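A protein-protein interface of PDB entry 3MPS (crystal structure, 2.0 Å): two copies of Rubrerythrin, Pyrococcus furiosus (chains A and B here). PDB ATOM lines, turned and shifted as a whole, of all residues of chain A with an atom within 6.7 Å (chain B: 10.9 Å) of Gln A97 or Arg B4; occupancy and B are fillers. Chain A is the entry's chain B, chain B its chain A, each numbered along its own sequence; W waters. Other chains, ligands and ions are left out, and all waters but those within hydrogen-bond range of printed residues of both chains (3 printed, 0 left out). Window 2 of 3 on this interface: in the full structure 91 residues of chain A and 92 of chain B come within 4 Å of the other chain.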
ATOM      1  N   LYS A  92     -15.229 -18.924  20.677  1.00  0.00           N
ATOM      2  CA  LYS A  92     -13.858 -19.048  21.211  1.00  0.00           C
ATOM      3  C   LYS A  92     -13.442 -17.788  21.997  1.00  0.00           C
ATOM      4  O   LYS A  92     -12.768 -17.877  23.023  1.00  0.00           O
ATOM      5  CB  LYS A  92     -12.854 -19.337  20.079  1.00  0.00           C
ATOM      6  CG  LYS A  92     -11.423 -19.645  20.551  1.00  0.00           C
ATOM      7  CD  LYS A  92     -11.134 -21.157  20.673  1.00  0.00           C
ATOM      8  CE  LYS A  92      -9.617 -21.405  20.812  1.00  0.00           C
ATOM      9  NZ  LYS A  92      -9.233 -22.806  21.225  1.00  0.00           N
ATOM     10  N   ALA A  93     -13.870 -16.627  21.509  1.00  0.00           N
ATOM     11  CA  ALA A  93     -13.598 -15.337  22.140  1.00  0.00           C
ATOM     12  C   ALA A  93     -14.245 -15.252  23.532  1.00  0.00           C
ATOM     13  O   ALA A  93     -13.569 -14.918  24.514  1.00  0.00           O
ATOM     14  CB  ALA A  93     -14.094 -14.207  21.250  1.00  0.00           C
ATOM     15  N   ALA A  94     -15.543 -15.571  23.589  1.00  0.00           N
ATOM     16  CA  ALA A  94     -16.313 -15.725  24.834  1.00  0.00           C
ATOM     17  C   ALA A  94     -15.642 -16.703  25.792  1.00  0.00           C
ATOM     18  O   ALA A  94     -15.555 -16.444  26.993  1.00  0.00           O
ATOM     19  CB  ALA A  94     -17.709 -16.221  24.518  1.00  0.00           C
ATOM     20  N   GLU A  95     -15.228 -17.842  25.246  1.00  0.00           N
ATOM     21  CA  GLU A  95     -14.499 -18.875  25.972  1.00  0.00           C
ATOM     22  C   GLU A  95     -13.264 -18.217  26.573  1.00  0.00           C
ATOM     23  O   GLU A  95     -13.099 -18.160  27.798  1.00  0.00           O
ATOM     24  CB  GLU A  95     -14.064 -19.975  24.994  1.00  0.00           C
ATOM     25  CG  GLU A  95     -14.348 -21.426  25.412  1.00  0.00           C
ATOM     26  CD  GLU A  95     -14.449 -22.369  24.199  1.00  0.00           C
ATOM     27  OE1 GLU A  95     -15.370 -23.224  24.155  1.00  0.00           O
ATOM     28  OE2 GLU A  95     -13.611 -22.244  23.278  1.00  0.00           O
ATOM     29  N   PHE A  96     -12.417 -17.700  25.685  1.00  0.00           N
ATOM     30  CA  PHE A  96     -11.155 -17.040  26.038  1.00  0.00           C
ATOM     31  C   PHE A  96     -11.364 -15.981  27.112  1.00  0.00           C
ATOM     32  O   PHE A  96     -10.514 -15.800  27.987  1.00  0.00           O
ATOM     33  CB  PHE A  96     -10.541 -16.436  24.767  1.00  0.00           C
ATOM     34  CG  PHE A  96      -9.327 -15.570  25.000  1.00  0.00           C
ATOM     35  CD1 PHE A  96      -9.384 -14.203  24.747  1.00  0.00           C
ATOM     36  CD2 PHE A  96      -8.123 -16.122  25.434  1.00  0.00           C
ATOM     37  CE1 PHE A  96      -8.272 -13.403  24.938  1.00  0.00           C
ATOM     38  CE2 PHE A  96      -7.001 -15.313  25.632  1.00  0.00           C
ATOM     39  CZ  PHE A  96      -7.081 -13.962  25.380  1.00  0.00           C
ATOM     40  N   GLN A  97     -12.499 -15.291  27.048  1.00  0.00           N
ATOM     41  CA  GLN A  97     -12.796 -14.206  27.975  1.00  0.00           C
ATOM     42  C   GLN A  97     -13.516 -14.683  29.232  1.00  0.00           C
ATOM     43  O   GLN A  97     -13.726 -13.905  30.172  1.00  0.00           O
ATOM     44  CB  GLN A  97     -13.558 -13.068  27.260  1.00  0.00           C
ATOM     45  CG  GLN A  97     -12.672 -12.284  26.281  1.00  0.00           C
ATOM     46  CD  GLN A  97     -13.094 -10.830  26.115  1.00  0.00           C
ATOM     47  OE1 GLN A  97     -14.263 -10.521  25.903  1.00  0.00           O
ATOM     48  NE2 GLN A  97     -12.128  -9.934  26.189  1.00  0.00           N
ATOM     49  N   GLY A  98     -13.871 -15.966  29.257  1.00  0.00           N
ATOM     50  CA  GLY A  98     -14.439 -16.586  30.458  1.00  0.00           C
ATOM     51  C   GLY A  98     -15.895 -16.259  30.687  1.00  0.00           C
ATOM     52  O   GLY A  98     -16.401 -16.400  31.810  1.00  0.00           O
ATOM     53  N   GLU A  99     -16.569 -15.812  29.632  1.00  0.00           N
ATOM     54  CA  GLU A  99     -17.951 -15.340  29.752  1.00  0.00           C
ATOM     55  C   GLU A  99     -18.896 -16.488  29.400  1.00  0.00           C
ATOM     56  O   GLU A  99     -19.164 -16.752  28.228  1.00  0.00           O
ATOM     57  CB  GLU A  99     -18.207 -14.100  28.879  1.00  0.00           C
ATOM     58  CG  GLU A  99     -17.522 -12.831  29.356  1.00  0.00           C
ATOM     59  CD  GLU A  99     -18.348 -12.053  30.378  1.00  0.00           C
ATOM     60  OE1 GLU A  99     -19.267 -12.643  30.989  1.00  0.00           O
ATOM     61  OE2 GLU A  99     -18.075 -10.844  30.555  1.00  0.00           O
ATOM     62  N   LYS A 100     -19.390 -17.161  30.430  1.00  0.00           N
ATOM     63  CA  LYS A 100     -20.083 -18.458  30.289  1.00  0.00           C
ATOM     64  C   LYS A 100     -21.459 -18.354  29.637  1.00  0.00           C
ATOM     65  O   LYS A 100     -21.885 -19.257  28.912  1.00  0.00           O
ATOM     66  CB  LYS A 100     -20.194 -19.161  31.650  1.00  0.00           C
ATOM     67  CG  LYS A 100     -18.864 -19.415  32.338  1.00  0.00           C
ATOM     68  CD  LYS A 100     -18.043 -20.503  31.635  1.00  0.00           C
ATOM     69  N   VAL B   1     -25.253 -11.328  33.243  1.00  0.00           N
ATOM     70  CA  VAL B   1     -24.882 -10.197  32.340  1.00  0.00           C
ATOM     71  C   VAL B   1     -23.437 -10.345  31.869  1.00  0.00           C
ATOM     72  O   VAL B   1     -22.530 -10.564  32.677  1.00  0.00           O
ATOM     73  CB  VAL B   1     -25.102  -8.822  33.029  1.00  0.00           C
ATOM     74  CG1 VAL B   1     -24.826  -7.662  32.053  1.00  0.00           C
ATOM     75  CG2 VAL B   1     -26.538  -8.725  33.584  1.00  0.00           C
ATOM     76  N   VAL B   2     -23.237 -10.270  30.552  1.00  0.00           N
ATOM     77  CA  VAL B   2     -21.906 -10.280  29.975  1.00  0.00           C
ATOM     78  C   VAL B   2     -21.264  -8.920  30.228  1.00  0.00           C
ATOM     79  O   VAL B   2     -21.881  -7.870  29.973  1.00  0.00           O
ATOM     80  CB  VAL B   2     -21.928 -10.592  28.450  1.00  0.00           C
ATOM     81  CG1 VAL B   2     -20.630 -10.165  27.811  1.00  0.00           C
ATOM     82  CG2 VAL B   2     -22.173 -12.079  28.209  1.00  0.00           C
ATOM     83  N   LYS B   3     -20.038  -8.956  30.750  1.00  0.00           N
ATOM     84  CA  LYS B   3     -19.321  -7.768  31.202  1.00  0.00           C
ATOM     85  C   LYS B   3     -18.091  -7.393  30.353  1.00  0.00           C
ATOM     86  O   LYS B   3     -17.830  -6.208  30.155  1.00  0.00           O
ATOM     87  CB  LYS B   3     -18.914  -7.909  32.685  1.00  0.00           C
ATOM     88  CG  LYS B   3     -20.009  -7.636  33.695  1.00  0.00           C
ATOM     89  CD  LYS B   3     -20.711  -8.922  34.113  1.00  0.00           C
ATOM     90  CE  LYS B   3     -21.603  -8.728  35.347  1.00  0.00           C
ATOM     91  NZ  LYS B   3     -20.832  -8.852  36.636  1.00  0.00           N
ATOM     92  N   ARG B   4     -17.335  -8.384  29.866  1.00  0.00           N
ATOM     93  CA  ARG B   4     -16.118  -8.110  29.077  1.00  0.00           C
ATOM     94  C   ARG B   4     -16.393  -7.429  27.730  1.00  0.00           C
ATOM     95  O   ARG B   4     -17.311  -7.821  27.006  1.00  0.00           O
ATOM     96  CB  ARG B   4     -15.285  -9.381  28.875  1.00  0.00           C
ATOM     97  CG  ARG B   4     -14.316  -9.643  30.016  1.00  0.00           C
ATOM     98  CD  ARG B   4     -13.067 -10.282  29.479  1.00  0.00           C
ATOM     99  NE  ARG B   4     -11.906 -10.082  30.336  1.00  0.00           N
ATOM    100  CZ  ARG B   4     -10.658 -10.373  29.982  1.00  0.00           C
ATOM    101  NH1 ARG B   4      -9.655 -10.156  30.831  1.00  0.00           N
ATOM    102  NH2 ARG B   4     -10.401 -10.879  28.782  1.00  0.00           N
ATOM    103  N   THR B   5     -15.575  -6.427  27.407  1.00  0.00           N
ATOM    104  CA  THR B   5     -15.845  -5.495  26.304  1.00  0.00           C
ATOM    105  C   THR B   5     -15.970  -6.181  24.937  1.00  0.00           C
ATOM    106  O   THR B   5     -16.952  -5.976  24.231  1.00  0.00           O
ATOM    107  CB  THR B   5     -14.802  -4.336  26.261  1.00  0.00           C
ATOM    108  OG1 THR B   5     -14.634  -3.799  27.579  1.00  0.00           O
ATOM    109  CG2 THR B   5     -15.269  -3.195  25.330  1.00  0.00           C
ATOM    110  N   MET B   6     -14.994  -7.005  24.583  1.00  0.00           N
ATOM    111  CA  MET B   6     -14.982  -7.646  23.255  1.00  0.00           C
ATOM    112  C   MET B   6     -16.170  -8.576  23.087  1.00  0.00           C
ATOM    113  O   MET B   6     -16.874  -8.513  22.075  1.00  0.00           O
ATOM    114  CB  MET B   6     -13.679  -8.426  23.036  1.00  0.00           C
ATOM    115  CG  MET B   6     -12.427  -7.559  22.928  1.00  0.00           C
ATOM    116  SD  MET B   6     -12.645  -6.053  21.947  1.00  0.00           S
ATOM    117  CE  MET B   6     -12.715  -6.698  20.254  1.00  0.00           C
ATOM    118  N   THR B   7     -16.390  -9.421  24.099  1.00  0.00           N
ATOM    119  CA  THR B   7     -17.501 -10.363  24.127  1.00  0.00           C
ATOM    120  C   THR B   7     -18.846  -9.639  24.086  1.00  0.00           C
ATOM    121  O   THR B   7     -19.754 -10.045  23.363  1.00  0.00           O
ATOM    122  CB  THR B   7     -17.414 -11.285  25.356  1.00  0.00           C
ATOM    123  OG1 THR B   7     -16.348 -12.224  25.166  1.00  0.00           O
ATOM    124  CG2 THR B   7     -18.702 -12.059  25.560  1.00  0.00           C
ATOM    125  N   LYS B   8     -18.964  -8.568  24.867  1.00  0.00           N
ATOM    126  CA  LYS B   8     -20.139  -7.722  24.821  1.00  0.00           C
ATOM    127  C   LYS B   8     -20.331  -7.157  23.422  1.00  0.00           C
ATOM    128  O   LYS B   8     -21.425  -7.272  22.879  1.00  0.00           O
ATOM    129  CB  LYS B   8     -20.054  -6.620  25.871  1.00  0.00           C
ATOM    130  CG  LYS B   8     -21.075  -5.528  25.724  1.00  0.00           C
ATOM    131  CD  LYS B   8     -21.194  -4.721  27.012  1.00  0.00           C
ATOM    132  CE  LYS B   8     -21.484  -3.256  26.711  1.00  0.00           C
ATOM    133  NZ  LYS B   8     -22.909  -2.994  26.315  1.00  0.00           N
ATOM    134  N   LYS B   9     -19.278  -6.561  22.845  1.00  0.00           N
ATOM    135  CA  LYS B   9     -19.320  -6.084  21.441  1.00  0.00           C
ATOM    136  C   LYS B   9     -19.753  -7.197  20.498  1.00  0.00           C
ATOM    137  O   LYS B   9     -20.594  -6.985  19.626  1.00  0.00           O
ATOM    138  CB  LYS B   9     -17.970  -5.506  20.968  1.00  0.00           C
ATOM    139  CG  LYS B   9     -17.810  -5.607  19.426  1.00  0.00           C
ATOM    140  CD  LYS B   9     -16.398  -5.339  18.879  1.00  0.00           C
ATOM    141  CE  LYS B   9     -16.399  -4.028  18.110  1.00  0.00           C
ATOM    142  NZ  LYS B   9     -15.648  -4.074  16.811  1.00  0.00           N
ATOM    143  N   PHE B  10     -19.200  -8.391  20.684  1.00  0.00           N
ATOM    144  CA  PHE B  10     -19.510  -9.520  19.790  1.00  0.00           C
ATOM    145  C   PHE B  10     -20.976  -9.962  19.900  1.00  0.00           C
ATOM    146  O   PHE B  10     -21.596 -10.241  18.896  1.00  0.00           O
ATOM    147  CB  PHE B  10     -18.558 -10.712  19.979  1.00  0.00           C
ATOM    148  CG  PHE B  10     -17.128 -10.457  19.544  1.00  0.00           C
ATOM    149  CD1 PHE B  10     -16.109 -11.260  20.027  1.00  0.00           C
ATOM    150  CD2 PHE B  10     -16.798  -9.428  18.668  1.00  0.00           C
ATOM    151  CE1 PHE B  10     -14.783 -11.051  19.654  1.00  0.00           C
ATOM    152  CE2 PHE B  10     -15.478  -9.210  18.291  1.00  0.00           C
ATOM    153  CZ  PHE B  10     -14.464 -10.022  18.778  1.00  0.00           C
ATOM    154  N   LEU B  11     -21.521  -9.997  21.121  1.00  0.00           N
ATOM    155  CA  LEU B  11     -22.930 -10.303  21.328  1.00  0.00           C
ATOM    156  C   LEU B  11     -23.858  -9.252  20.742  1.00  0.00           C
ATOM    157  O   LEU B  11     -24.949  -9.579  20.300  1.00  0.00           O
ATOM    158  CB  LEU B  11     -23.233 -10.482  22.825  1.00  0.00           C
ATOM    159  CG  LEU B  11     -22.769 -11.778  23.502  1.00  0.00           C
ATOM    160  CD1 LEU B  11     -23.547 -11.988  24.795  1.00  0.00           C
ATOM    161  CD2 LEU B  11     -22.976 -12.977  22.604  1.00  0.00           C
ATOM    162  N   GLU B  12     -23.430  -7.990  20.776  1.00  0.00           N
ATOM    163  CA  GLU B  12     -24.186  -6.887  20.204  1.00  0.00           C
ATOM    164  C   GLU B  12     -24.244  -7.018  18.668  1.00  0.00           C
ATOM    165  O   GLU B  12     -25.298  -6.813  18.058  1.00  0.00           O
ATOM    166  CB  GLU B  12     -23.583  -5.549  20.621  1.00  0.00           C
ATOM    167  CG  GLU B  12     -23.819  -5.164  22.101  1.00  0.00           C
ATOM    168  CD  GLU B  12     -22.959  -4.004  22.549  1.00  0.00           C
ATOM    169  OE1 GLU B  12     -22.259  -3.412  21.701  1.00  0.00           O
ATOM    170  OE2 GLU B  12     -22.964  -3.680  23.762  1.00  0.00           O
ATOM    171  N   GLU B  13     -23.116  -7.391  18.076  1.00  0.00           N
ATOM    172  CA  GLU B  13     -23.005  -7.681  16.632  1.00  0.00           C
ATOM    173  C   GLU B  13     -23.886  -8.837  16.206  1.00  0.00           C
ATOM    174  O   GLU B  13     -24.676  -8.719  15.256  1.00  0.00           O
ATOM    175  CB  GLU B  13     -21.571  -8.046  16.285  1.00  0.00           C
ATOM    176  CG  GLU B  13     -20.528  -7.160  16.875  1.00  0.00           C
ATOM    177  CD  GLU B  13     -19.745  -6.399  15.840  1.00  0.00           C
ATOM    178  OE1 GLU B  13     -20.303  -6.129  14.748  1.00  0.00           O
ATOM    179  OE2 GLU B  13     -18.571  -6.071  16.127  1.00  0.00           O
ATOM    180  N   ALA B  61     -28.454 -12.294  27.476  1.00  0.00           N
ATOM    181  CA  ALA B  61     -27.062 -12.402  27.916  1.00  0.00           C
ATOM    182  C   ALA B  61     -26.405 -11.043  28.153  1.00  0.00           C
ATOM    183  O   ALA B  61     -25.632 -10.896  29.100  1.00  0.00           O
ATOM    184  CB  ALA B  61     -26.235 -13.244  26.924  1.00  0.00           C
ATOM    185  N   LEU B  62     -26.721 -10.049  27.311  1.00  0.00           N
ATOM    186  CA  LEU B  62     -26.218  -8.674  27.502  1.00  0.00           C
ATOM    187  C   LEU B  62     -26.915  -7.963  28.679  1.00  0.00           C
ATOM    188  O   LEU B  62     -26.480  -6.896  29.090  1.00  0.00           O
ATOM    189  CB  LEU B  62     -26.344  -7.837  26.212  1.00  0.00           C
ATOM    190  CG  LEU B  62     -25.522  -8.350  25.010  1.00  0.00           C
ATOM    191  CD1 LEU B  62     -26.181  -8.131  23.648  1.00  0.00           C
ATOM    192  CD2 LEU B  62     -24.129  -7.783  25.060  1.00  0.00           C
ATOM    193  N   GLY B  63     -27.983  -8.566  29.206  1.00  0.00           N
ATOM    194  CA  GLY B  63     -28.746  -7.987  30.338  1.00  0.00           C
ATOM    195  C   GLY B  63     -29.702  -6.887  29.899  1.00  0.00           C
ATOM    196  O   GLY B  63     -30.002  -5.961  30.656  1.00  0.00           O
ATOM    197  N   LYS B  64     -30.203  -6.999  28.674  1.00  0.00           N
ATOM    198  CA  LYS B  64     -31.048  -5.942  28.098  1.00  0.00           C
ATOM    199  C   LYS B  64     -32.554  -6.147  28.261  1.00  0.00           C
ATOM    200  O   LYS B  64     -33.342  -5.230  27.973  1.00  0.00           O
ATOM    201  CB  LYS B  64     -30.681  -5.717  26.617  1.00  0.00           C
ATOM    202  CG  LYS B  64     -29.229  -5.259  26.372  1.00  0.00           C
ATOM    203  CD  LYS B  64     -28.840  -3.992  27.176  1.00  0.00           C
ATOM    204  CE  LYS B  64     -27.401  -3.524  26.838  1.00  0.00           C
ATOM    205  NZ  LYS B  64     -26.629  -2.932  27.997  1.00  0.00           N
HETATM  206  O   HOH W   1      -9.165 -13.914  29.271  1.00  0.00           O
HETATM  207  O   HOH W   2     -20.412 -12.120  33.226  1.00  0.00           O
HETATM  208  O   HOH W   3      -8.914 -10.277  26.614  1.00  0.00           O
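Of the printed residues of chain B, Gln A97 touches Arg B4 (3.3 Å), Met B6 (3.6 Å) and Thr B7 (2.8 Å).
Of chain A, only Gln A97 (3.3 Å) and Glu A99 (2.7 Å) come within 4 Å of Arg B4.
Of chain B, only Thr B7 (3.9 Å) and Phe B10 (3.6 Å) come within 4 Å of Ala A93.
Gly A98 touches none of the printed residues of chain B.
Glu A99 touches four residues of chain B.
Of the printed residues of chain A, Val B2 touches Glu A99 (3.7 Å).
Of the printed residues of chain A, Phe B10 touches Ala A93.
Lys B64 touches none of the printed residues of chain A.
The nearest residue of chain B that does not touch Gln A97 is Thr B5 (4.6 Å).
The backbone NH (N) of Val B2 is in hydrogen-bond range of the backbone carbonyl oxygen (O) of Ala B61.
The backbone carbonyl oxygen (O) of Ala A94 lies within hydrogen-bond range of the backbone NH (N) of Glu A99.
The backbone NH (N) of Lys B3 lies within hydrogen-bond range of the side-chain carboxylate (OE2) of Glu A99, 2.7 Å away.
The guanidinium group (NH2) of Arg B4 lies close to the side-chain amide nitrogen (NE2) of Gln A97, 3.3 Å away.
The backbone NH of Arg B4 is in hydrogen-bond range of the side-chain carboxylate of Glu A99 (2.7 Å).
OE1 of Gln A97 sits at hydrogen-bond distance from OG1 of Thr B7 (2.8 Å).
No position is printed for both chains.
Of the 10 pairs that touch across the chains among the printed residues, none has its exchanged pair printed and touching as well.
Hydrophobic or aromatic side chains of chain A that line the printed part of chain B: Ala A93.
Printed residues of chain B that touch a printed residue of chain A: Val B2, Lys B3, Arg B4, Met B6, Thr B7 and Phe B10.
Hydrophobic or aromatic side chains of chain B that line the printed part of chain A: Val B2, Met B6 and Phe B10.
Water W2 lies within hydrogen-bond range of OE1 of Glu A99 and O of Val B1.
Water W1 lies within hydrogen-bond range of the backbone carbonyl oxygen of Phe A96 and the guanidinium group of Arg B4.
Water W3 lies within hydrogen-bond range of NH2 of Arg B4 and NE2 of Gln A97.
Thr B7 touches Ala A93 (OG1 to O, 3.9 Å).
CE1 of Phe B10 touches CB of Ala A93 (3.6 Å).
CA of Ala A94 touches OG1 of Thr B7, at 3.5 Å.
Met B6 touches Gln A97 (CB to OE1, 3.6 Å).
Val B2 touches Glu A99.
Glu A99 touches Thr B7.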
